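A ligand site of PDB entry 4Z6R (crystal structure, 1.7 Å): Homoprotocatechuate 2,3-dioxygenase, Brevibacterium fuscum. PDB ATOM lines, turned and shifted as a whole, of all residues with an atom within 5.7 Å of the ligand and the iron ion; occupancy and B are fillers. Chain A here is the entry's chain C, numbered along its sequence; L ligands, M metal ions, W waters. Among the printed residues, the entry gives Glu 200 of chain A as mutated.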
ATOM      1  N   HIS A 155      15.718   3.359 -15.358  1.00  0.00           N
ATOM      2  CA  HIS A 155      15.663   4.071 -16.634  1.00  0.00           C
ATOM      3  C   HIS A 155      14.602   5.140 -16.688  1.00  0.00           C
ATOM      4  O   HIS A 155      13.791   5.275 -15.754  1.00  0.00           O
ATOM      5  CB  HIS A 155      15.339   3.057 -17.751  1.00  0.00           C
ATOM      6  CG  HIS A 155      13.988   2.426 -17.616  1.00  0.00           C
ATOM      7  ND1 HIS A 155      13.787   1.181 -17.034  1.00  0.00           N
ATOM      8  CD2 HIS A 155      12.771   2.831 -18.044  1.00  0.00           C
ATOM      9  CE1 HIS A 155      12.515   0.850 -17.134  1.00  0.00           C
ATOM     10  NE2 HIS A 155      11.882   1.837 -17.735  1.00  0.00           N
ATOM     11  N   ASN A 157      11.726   6.975 -19.578  1.00  0.00           N
ATOM     12  CA  ASN A 157      10.982   6.765 -20.806  1.00  0.00           C
ATOM     13  C   ASN A 157      10.395   8.118 -21.224  1.00  0.00           C
ATOM     14  O   ASN A 157       9.749   8.746 -20.448  1.00  0.00           O
ATOM     15  CB  ASN A 157       9.898   5.713 -20.629  1.00  0.00           C
ATOM     16  CG  ASN A 157       9.245   5.320 -21.945  1.00  0.00           C
ATOM     17  OD1 ASN A 157       8.706   6.135 -22.664  1.00  0.00           O
ATOM     18  ND2 ASN A 157       9.311   4.059 -22.268  1.00  0.00           N
ATOM     19  N   ILE A 181       9.151  -1.732 -31.370  1.00  0.00           N
ATOM     20  CA  ILE A 181       7.830  -2.117 -31.848  1.00  0.00           C
ATOM     21  C   ILE A 181       7.551  -1.415 -33.197  1.00  0.00           C
ATOM     22  O   ILE A 181       7.614  -0.172 -33.273  1.00  0.00           O
ATOM     23  CB  ILE A 181       6.739  -1.679 -30.853  1.00  0.00           C
ATOM     24  CG1 ILE A 181       6.893  -2.412 -29.542  1.00  0.00           C
ATOM     25  CG2 ILE A 181       5.343  -1.923 -31.428  1.00  0.00           C
ATOM     26  CD1 ILE A 181       6.073  -1.867 -28.380  1.00  0.00           C
ATOM     27  N   TRP A 192      13.711   0.906 -27.334  1.00  0.00           N
ATOM     28  CA  TRP A 192      14.392   0.858 -26.037  1.00  0.00           C
ATOM     29  C   TRP A 192      15.896   0.787 -26.278  1.00  0.00           C
ATOM     30  O   TRP A 192      16.316   0.120 -27.177  1.00  0.00           O
ATOM     31  CB  TRP A 192      13.971  -0.429 -25.335  1.00  0.00           C
ATOM     32  CG  TRP A 192      12.553  -0.362 -24.766  1.00  0.00           C
ATOM     33  CD1 TRP A 192      12.251  -0.231 -23.454  1.00  0.00           C
ATOM     34  CD2 TRP A 192      11.291  -0.449 -25.465  1.00  0.00           C
ATOM     35  NE1 TRP A 192      10.873  -0.228 -23.275  1.00  0.00           N
ATOM     36  CE2 TRP A 192      10.258  -0.376 -24.484  1.00  0.00           C
ATOM     37  CE3 TRP A 192      10.915  -0.622 -26.808  1.00  0.00           C
ATOM     38  CZ2 TRP A 192       8.911  -0.447 -24.802  1.00  0.00           C
ATOM     39  CZ3 TRP A 192       9.532  -0.684 -27.126  1.00  0.00           C
ATOM     40  CH2 TRP A 192       8.559  -0.600 -26.111  1.00  0.00           C
ATOM     41  N   GLU A 200      17.387  -1.057 -20.983  1.00  0.00           N
ATOM     42  CA  GLU A 200      17.227   0.385 -21.219  1.00  0.00           C
ATOM     43  C   GLU A 200      17.884   1.248 -20.159  1.00  0.00           C
ATOM     44  O   GLU A 200      17.881   0.892 -18.970  1.00  0.00           O
ATOM     45  CB  GLU A 200      15.719   0.725 -21.243  1.00  0.00           C
ATOM     46  CG  GLU A 200      14.949  -0.035 -20.129  1.00  0.00           C
ATOM     47  CD  GLU A 200      13.426   0.115 -20.234  1.00  0.00           C
ATOM     48  OE1 GLU A 200      12.978   1.227 -20.686  1.00  0.00           O
ATOM     49  OE2 GLU A 200      12.693  -0.875 -19.876  1.00  0.00           O
ATOM     50  N   HIS A 214       7.703   8.149 -17.897  1.00  0.00           N
ATOM     51  CA  HIS A 214       7.904   7.668 -16.557  1.00  0.00           C
ATOM     52  C   HIS A 214       9.358   7.664 -16.203  1.00  0.00           C
ATOM     53  O   HIS A 214      10.255   7.743 -17.085  1.00  0.00           O
ATOM     54  CB  HIS A 214       7.293   6.243 -16.329  1.00  0.00           C
ATOM     55  CG  HIS A 214       7.845   5.165 -17.195  1.00  0.00           C
ATOM     56  ND1 HIS A 214       7.219   4.759 -18.347  1.00  0.00           N
ATOM     57  CD2 HIS A 214       8.886   4.317 -17.026  1.00  0.00           C
ATOM     58  CE1 HIS A 214       7.878   3.758 -18.906  1.00  0.00           C
ATOM     59  NE2 HIS A 214       8.897   3.468 -18.110  1.00  0.00           N
ATOM     60  N   ALA A 216      11.694   4.877 -13.865  1.00  0.00           N
ATOM     61  CA  ALA A 216      11.625   3.471 -13.390  1.00  0.00           C
ATOM     62  C   ALA A 216      12.680   3.157 -12.359  1.00  0.00           C
ATOM     63  O   ALA A 216      13.875   3.419 -12.559  1.00  0.00           O
ATOM     64  CB  ALA A 216      11.737   2.514 -14.543  1.00  0.00           C
ATOM     65  N   ARG A 243      -1.582   0.716 -14.082  1.00  0.00           N
ATOM     66  CA  ARG A 243      -1.427  -0.438 -14.976  1.00  0.00           C
ATOM     67  C   ARG A 243      -0.511  -1.447 -14.340  1.00  0.00           C
ATOM     68  O   ARG A 243       0.518  -1.115 -13.817  1.00  0.00           O
ATOM     69  CB  ARG A 243      -0.789   0.018 -16.282  1.00  0.00           C
ATOM     70  CG  ARG A 243      -0.404  -1.107 -17.249  1.00  0.00           C
ATOM     71  CD  ARG A 243       0.045  -0.614 -18.599  1.00  0.00           C
ATOM     72  NE  ARG A 243       0.548  -1.800 -19.301  1.00  0.00           N
ATOM     73  CZ  ARG A 243       1.646  -1.853 -20.047  1.00  0.00           C
ATOM     74  NH1 ARG A 243       2.285  -0.744 -20.461  1.00  0.00           N
ATOM     75  NH2 ARG A 243       2.049  -3.002 -20.473  1.00  0.00           N
ATOM     76  N   HIS A 248       6.188  -7.841 -18.861  1.00  0.00           N
ATOM     77  CA  HIS A 248       6.319  -7.159 -20.151  1.00  0.00           C
ATOM     78  C   HIS A 248       6.684  -8.191 -21.215  1.00  0.00           C
ATOM     79  O   HIS A 248       7.334  -9.232 -20.924  1.00  0.00           O
ATOM     80  CB  HIS A 248       7.435  -6.136 -20.146  1.00  0.00           C
ATOM     81  CG  HIS A 248       7.119  -4.832 -19.529  1.00  0.00           C
ATOM     82  ND1 HIS A 248       5.986  -4.122 -19.846  1.00  0.00           N
ATOM     83  CD2 HIS A 248       7.805  -4.080 -18.634  1.00  0.00           C
ATOM     84  CE1 HIS A 248       5.990  -2.971 -19.197  1.00  0.00           C
ATOM     85  NE2 HIS A 248       7.095  -2.915 -18.475  1.00  0.00           N
ATOM     86  N   GLY A 249       6.278  -7.932 -22.448  1.00  0.00           N
ATOM     87  CA  GLY A 249       6.862  -8.634 -23.593  1.00  0.00           C
ATOM     88  C   GLY A 249       8.230  -8.053 -23.891  1.00  0.00           C
ATOM     89  O   GLY A 249       9.279  -8.635 -23.545  1.00  0.00           O
ATOM     90  N   VAL A 250       8.215  -6.834 -24.428  1.00  0.00           N
ATOM     91  CA  VAL A 250       9.424  -6.058 -24.518  1.00  0.00           C
ATOM     92  C   VAL A 250      10.078  -5.930 -23.143  1.00  0.00           C
ATOM     93  O   VAL A 250       9.459  -5.478 -22.214  1.00  0.00           O
ATOM     94  CB  VAL A 250       9.152  -4.627 -25.029  1.00  0.00           C
ATOM     95  CG1 VAL A 250      10.455  -3.819 -25.047  1.00  0.00           C
ATOM     96  CG2 VAL A 250       8.495  -4.664 -26.408  1.00  0.00           C
ATOM     97  N   SER A 251      11.312  -6.395 -23.042  1.00  0.00           N
ATOM     98  CA  SER A 251      12.160  -6.348 -21.849  1.00  0.00           C
ATOM     99  C   SER A 251      12.046  -7.592 -20.983  1.00  0.00           C
ATOM    100  O   SER A 251      12.979  -7.871 -20.246  1.00  0.00           O
ATOM    101  CB  SER A 251      11.969  -5.122 -20.971  1.00  0.00           C
ATOM    102  OG  SER A 251      10.903  -5.249 -20.059  1.00  0.00           O
ATOM    103  N   TYR A 255       6.524  -5.843 -13.922  1.00  0.00           N
ATOM    104  CA  TYR A 255       6.360  -4.378 -13.905  1.00  0.00           C
ATOM    105  C   TYR A 255       5.104  -3.952 -13.174  1.00  0.00           C
ATOM    106  O   TYR A 255       4.143  -4.719 -13.014  1.00  0.00           O
ATOM    107  CB  TYR A 255       6.321  -3.762 -15.307  1.00  0.00           C
ATOM    108  CG  TYR A 255       5.035  -4.060 -16.066  1.00  0.00           C
ATOM    109  CD1 TYR A 255       3.925  -3.238 -15.976  1.00  0.00           C
ATOM    110  CD2 TYR A 255       4.959  -5.190 -16.884  1.00  0.00           C
ATOM    111  CE1 TYR A 255       2.762  -3.509 -16.651  1.00  0.00           C
ATOM    112  CE2 TYR A 255       3.777  -5.471 -17.585  1.00  0.00           C
ATOM    113  CZ  TYR A 255       2.682  -4.623 -17.488  1.00  0.00           C
ATOM    114  OH  TYR A 255       1.509  -4.923 -18.158  1.00  0.00           O
ATOM    115  N   TYR A 257       2.975   0.181 -12.956  1.00  0.00           N
ATOM    116  CA  TYR A 257       2.961   1.636 -13.105  1.00  0.00           C
ATOM    117  C   TYR A 257       2.017   2.290 -12.066  1.00  0.00           C
ATOM    118  O   TYR A 257       0.830   1.923 -11.975  1.00  0.00           O
ATOM    119  CB  TYR A 257       2.519   2.057 -14.490  1.00  0.00           C
ATOM    120  CG  TYR A 257       3.426   1.568 -15.596  1.00  0.00           C
ATOM    121  CD1 TYR A 257       4.578   2.298 -15.967  1.00  0.00           C
ATOM    122  CD2 TYR A 257       3.162   0.379 -16.241  1.00  0.00           C
ATOM    123  CE1 TYR A 257       5.413   1.776 -16.952  1.00  0.00           C
ATOM    124  CE2 TYR A 257       3.969  -0.112 -17.248  1.00  0.00           C
ATOM    125  CZ  TYR A 257       5.078   0.590 -17.616  1.00  0.00           C
ATOM    126  OH  TYR A 257       5.876   0.043 -18.632  1.00  0.00           O
ATOM    127  N   GLU A 267       7.376   3.766 -12.857  1.00  0.00           N
ATOM    128  CA  GLU A 267       7.398   2.310 -13.081  1.00  0.00           C
ATOM    129  C   GLU A 267       8.236   1.609 -11.996  1.00  0.00           C
ATOM    130  O   GLU A 267       9.353   2.051 -11.667  1.00  0.00           O
ATOM    131  CB  GLU A 267       7.924   1.953 -14.477  1.00  0.00           C
ATOM    132  CG  GLU A 267       7.827   0.454 -14.766  1.00  0.00           C
ATOM    133  CD  GLU A 267       8.368   0.041 -16.111  1.00  0.00           C
ATOM    134  OE1 GLU A 267       9.143   0.813 -16.670  1.00  0.00           O
ATOM    135  OE2 GLU A 267       7.988  -1.031 -16.603  1.00  0.00           O
ATOM    136  N   TYR A 269      10.002  -2.243 -11.594  1.00  0.00           N
ATOM    137  CA  TYR A 269      10.524  -3.068 -12.673  1.00  0.00           C
ATOM    138  C   TYR A 269      11.508  -4.073 -12.077  1.00  0.00           C
ATOM    139  O   TYR A 269      12.329  -3.716 -11.224  1.00  0.00           O
ATOM    140  CB  TYR A 269      11.315  -2.102 -13.551  1.00  0.00           C
ATOM    141  CG  TYR A 269      11.910  -2.542 -14.861  1.00  0.00           C
ATOM    142  CD1 TYR A 269      11.175  -2.483 -16.019  1.00  0.00           C
ATOM    143  CD2 TYR A 269      13.279  -2.914 -14.953  1.00  0.00           C
ATOM    144  CE1 TYR A 269      11.754  -2.760 -17.266  1.00  0.00           C
ATOM    145  CE2 TYR A 269      13.844  -3.217 -16.206  1.00  0.00           C
ATOM    146  CZ  TYR A 269      13.065  -3.115 -17.340  1.00  0.00           C
ATOM    147  OH  TYR A 269      13.670  -3.388 -18.572  1.00  0.00           O
ATOM    148  N   ARG A 292       2.974  -8.061 -26.624  1.00  0.00           N
ATOM    149  CA  ARG A 292       4.206  -7.239 -26.728  1.00  0.00           C
ATOM    150  C   ARG A 292       4.408  -6.356 -25.516  1.00  0.00           C
ATOM    151  O   ARG A 292       5.535  -6.090 -25.152  1.00  0.00           O
ATOM    152  CB  ARG A 292       4.213  -6.361 -28.000  1.00  0.00           C
ATOM    153  CG  ARG A 292       3.351  -5.066 -27.919  1.00  0.00           C
ATOM    154  CD  ARG A 292       2.881  -4.455 -29.269  1.00  0.00           C
ATOM    155  NE  ARG A 292       1.987  -3.346 -28.945  1.00  0.00           N
ATOM    156  CZ  ARG A 292       0.709  -3.441 -28.539  1.00  0.00           C
ATOM    157  NH1 ARG A 292       0.044  -4.620 -28.562  1.00  0.00           N
ATOM    158  NH2 ARG A 292       0.071  -2.343 -28.175  1.00  0.00           N
ATOM    159  N   ARG A 293       3.315  -5.866 -24.933  1.00  0.00           N
ATOM    160  CA  ARG A 293       3.405  -4.902 -23.816  1.00  0.00           C
ATOM    161  C   ARG A 293       3.111  -5.589 -22.457  1.00  0.00           C
ATOM    162  O   ARG A 293       3.894  -5.500 -21.516  1.00  0.00           O
ATOM    163  CB  ARG A 293       2.495  -3.661 -24.051  1.00  0.00           C
ATOM    164  CG  ARG A 293       3.087  -2.710 -25.089  1.00  0.00           C
ATOM    165  CD  ARG A 293       2.573  -1.287 -24.988  1.00  0.00           C
ATOM    166  NE  ARG A 293       3.247  -0.344 -25.919  1.00  0.00           N
ATOM    167  CZ  ARG A 293       4.385   0.321 -25.698  1.00  0.00           C
ATOM    168  NH1 ARG A 293       5.161   0.131 -24.635  1.00  0.00           N
ATOM    169  NH2 ARG A 293       4.786   1.177 -26.629  1.00  0.00           N
ATOM    170  N   ASP A 294       2.015  -6.301 -22.404  1.00  0.00           N
ATOM    171  CA  ASP A 294       1.813  -7.224 -21.330  1.00  0.00           C
ATOM    172  C   ASP A 294       1.784  -8.645 -21.935  1.00  0.00           C
ATOM    173  O   ASP A 294       0.944  -9.009 -22.752  1.00  0.00           O
ATOM    174  CB  ASP A 294       0.540  -6.876 -20.586  1.00  0.00           C
ATOM    175  CG  ASP A 294       0.343  -7.675 -19.349  1.00  0.00           C
ATOM    176  OD1 ASP A 294       0.856  -7.255 -18.291  1.00  0.00           O
ATOM    177  OD2 ASP A 294      -0.279  -8.774 -19.433  1.00  0.00           O
ATOM    178  N   TRP A 304      -2.336   5.270 -20.250  1.00  0.00           N
ATOM    179  CA  TRP A 304      -0.941   4.935 -20.421  1.00  0.00           C
ATOM    180  C   TRP A 304      -0.325   5.487 -21.736  1.00  0.00           C
ATOM    181  O   TRP A 304       0.830   5.873 -21.819  1.00  0.00           O
ATOM    182  CB  TRP A 304      -0.777   3.404 -20.314  1.00  0.00           C
ATOM    183  CG  TRP A 304       0.638   3.008 -19.997  1.00  0.00           C
ATOM    184  CD1 TRP A 304       1.190   2.889 -18.758  1.00  0.00           C
ATOM    185  CD2 TRP A 304       1.705   2.743 -20.938  1.00  0.00           C
ATOM    186  NE1 TRP A 304       2.516   2.531 -18.839  1.00  0.00           N
ATOM    187  CE2 TRP A 304       2.857   2.443 -20.171  1.00  0.00           C
ATOM    188  CE3 TRP A 304       1.779   2.755 -22.318  1.00  0.00           C
ATOM    189  CZ2 TRP A 304       4.071   2.143 -20.760  1.00  0.00           C
ATOM    190  CZ3 TRP A 304       2.969   2.457 -22.905  1.00  0.00           C
ATOM    191  CH2 TRP A 304       4.117   2.166 -22.135  1.00  0.00           C
HETATM  192  O1  LIG L   1       4.695  -2.032 -21.961  1.00  0.00           O
HETATM  193  S1  LIG L   1       6.100  -2.545 -22.643  1.00  0.00           S
HETATM  194  O2  LIG L   1       6.248  -4.049 -22.663  1.00  0.00           O
HETATM  195  O3  LIG L   1       6.234  -2.051 -24.029  1.00  0.00           O
HETATM  196  C1  LIG L   1       7.448  -1.867 -21.820  1.00  0.00           C
HETATM  197  C2  LIG L   1       7.263  -0.578 -21.247  1.00  0.00           C
HETATM  198  C3  LIG L   1       8.633  -2.594 -21.656  1.00  0.00           C
HETATM  199  C4  LIG L   1       9.642  -2.076 -20.817  1.00  0.00           C
HETATM  200  C5  LIG L   1       9.422  -0.905 -20.102  1.00  0.00           C
HETATM  201  O4  LIG L   1      10.359  -0.423 -19.204  1.00  0.00           O
HETATM  202  C6  LIG L   1       8.209  -0.169 -20.322  1.00  0.00           C
HETATM  203  O5  LIG L   1       7.939   0.904 -19.571  1.00  0.00           O
HETATM  204 FE    FE M   1       9.745   1.482 -18.564  1.00  0.00          FE
HETATM  205  O   HOH W   1      10.347   2.049 -20.679  1.00  0.00           O
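O of Arg 292 lies close to O2 of the ligand (3.3 Å). Trp 192 touches the ligand (CZ2 to O3, 3.2 Å). Gly 249 touches the ligand. Val 250 touches the ligand (O to C3, 3.1 Å). Ser 251 touches the ligand (OG to C4, 3.5 Å). Tyr 269 touches the ligand. Hydrophobic or aromatic side chains that line the ligand: His 155, Trp 192, His 214, His 248, Val 250, Tyr 257 and Tyr 269. 14 residues have an atom within 4 Å of the ligand: His 155, Trp 192, Glu 200, His 214, Arg 243, His 248, Gly 249, Val 250, Ser 251, Tyr 257, Glu 267, Tyr 269, Arg 292 and Arg 293.
OH of Tyr 257 sits close to O5 of the ligand (2.4 Å). O of Arg 293 sits close to O2 of the ligand. O3 of the ligand is in salt-bridge range of NH1 of Arg 293. A ring nitrogen (ND1) of His 248 lies within hydrogen-bond range of an oxygen (O2) of the ligand, 2.8 Å away. An oxygen (O1) of the ligand lies within salt-bridge range of the guanidinium group (NH1) of Arg 243 (3.1 Å). An oxygen (O4) of the ligand lies close to the side-chain carboxylate (OE2) of Glu 200 (2.5 Å).
Water W1 lies within hydrogen-bond range of OE1 of Glu 200 (2.8 Å), ND2 of Asn 157 (2.8 Å) and NE1 of Trp 192 (3.5 Å).
The iron ion is bound by the side-chain carboxylate (OE1) of Glu 267 (2.1 Å), an oxygen (O4) of the ligand (2.1 Å), an oxygen (O5) of the ligand (2.1 Å), a ring nitrogen (NE2) of His 214 (2.2 Å), water W1 (2.3 Å) and a ring nitrogen (NE2) of His 155 (2.3 Å). The iron ion has six donor atoms within binding distance.
NH2 of Arg 243 sits at hydrogen-bond distance from OH of Tyr 255, 3.1 Å away. O of His 214 sits at hydrogen-bond distance from N of Asn 157 (3.0 Å). OH of Tyr 269 lies within hydrogen-bond range of OE2 of Glu 200 (3.0 Å). The side-chain hydroxyl (OH) of Tyr 257 sits close to a ring nitrogen (NE2) of His 248, 3.2 Å away. The backbone carbonyl oxygen (O) of Arg 293 sits at hydrogen-bond distance from a ring nitrogen (ND1) of His 248. The side-chain carboxylate (OE2) of Glu 267 sits at hydrogen-bond distance from the side-chain hydroxyl (OH) of Tyr 257. The backbone NH (N) of Gly 249 sits close to the backbone carbonyl oxygen (O) of Arg 292, at 3.4 Å. The backbone carbonyl oxygen (O) of Arg 293 sits at hydrogen-bond distance from the guanidinium group (NH2) of Arg 243 (3.3 Å).
Glu 200 touches the iron ion (OE1 to FE, 3.9 Å). Of the 20 residues printed, 4 come within 4 Å of the iron ion. Along chain A the residues within 4 Å of the iron ion span positions 155 to 267. The nearest printed residue that does not touch the iron ion is Tyr 257 (4.1 Å).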
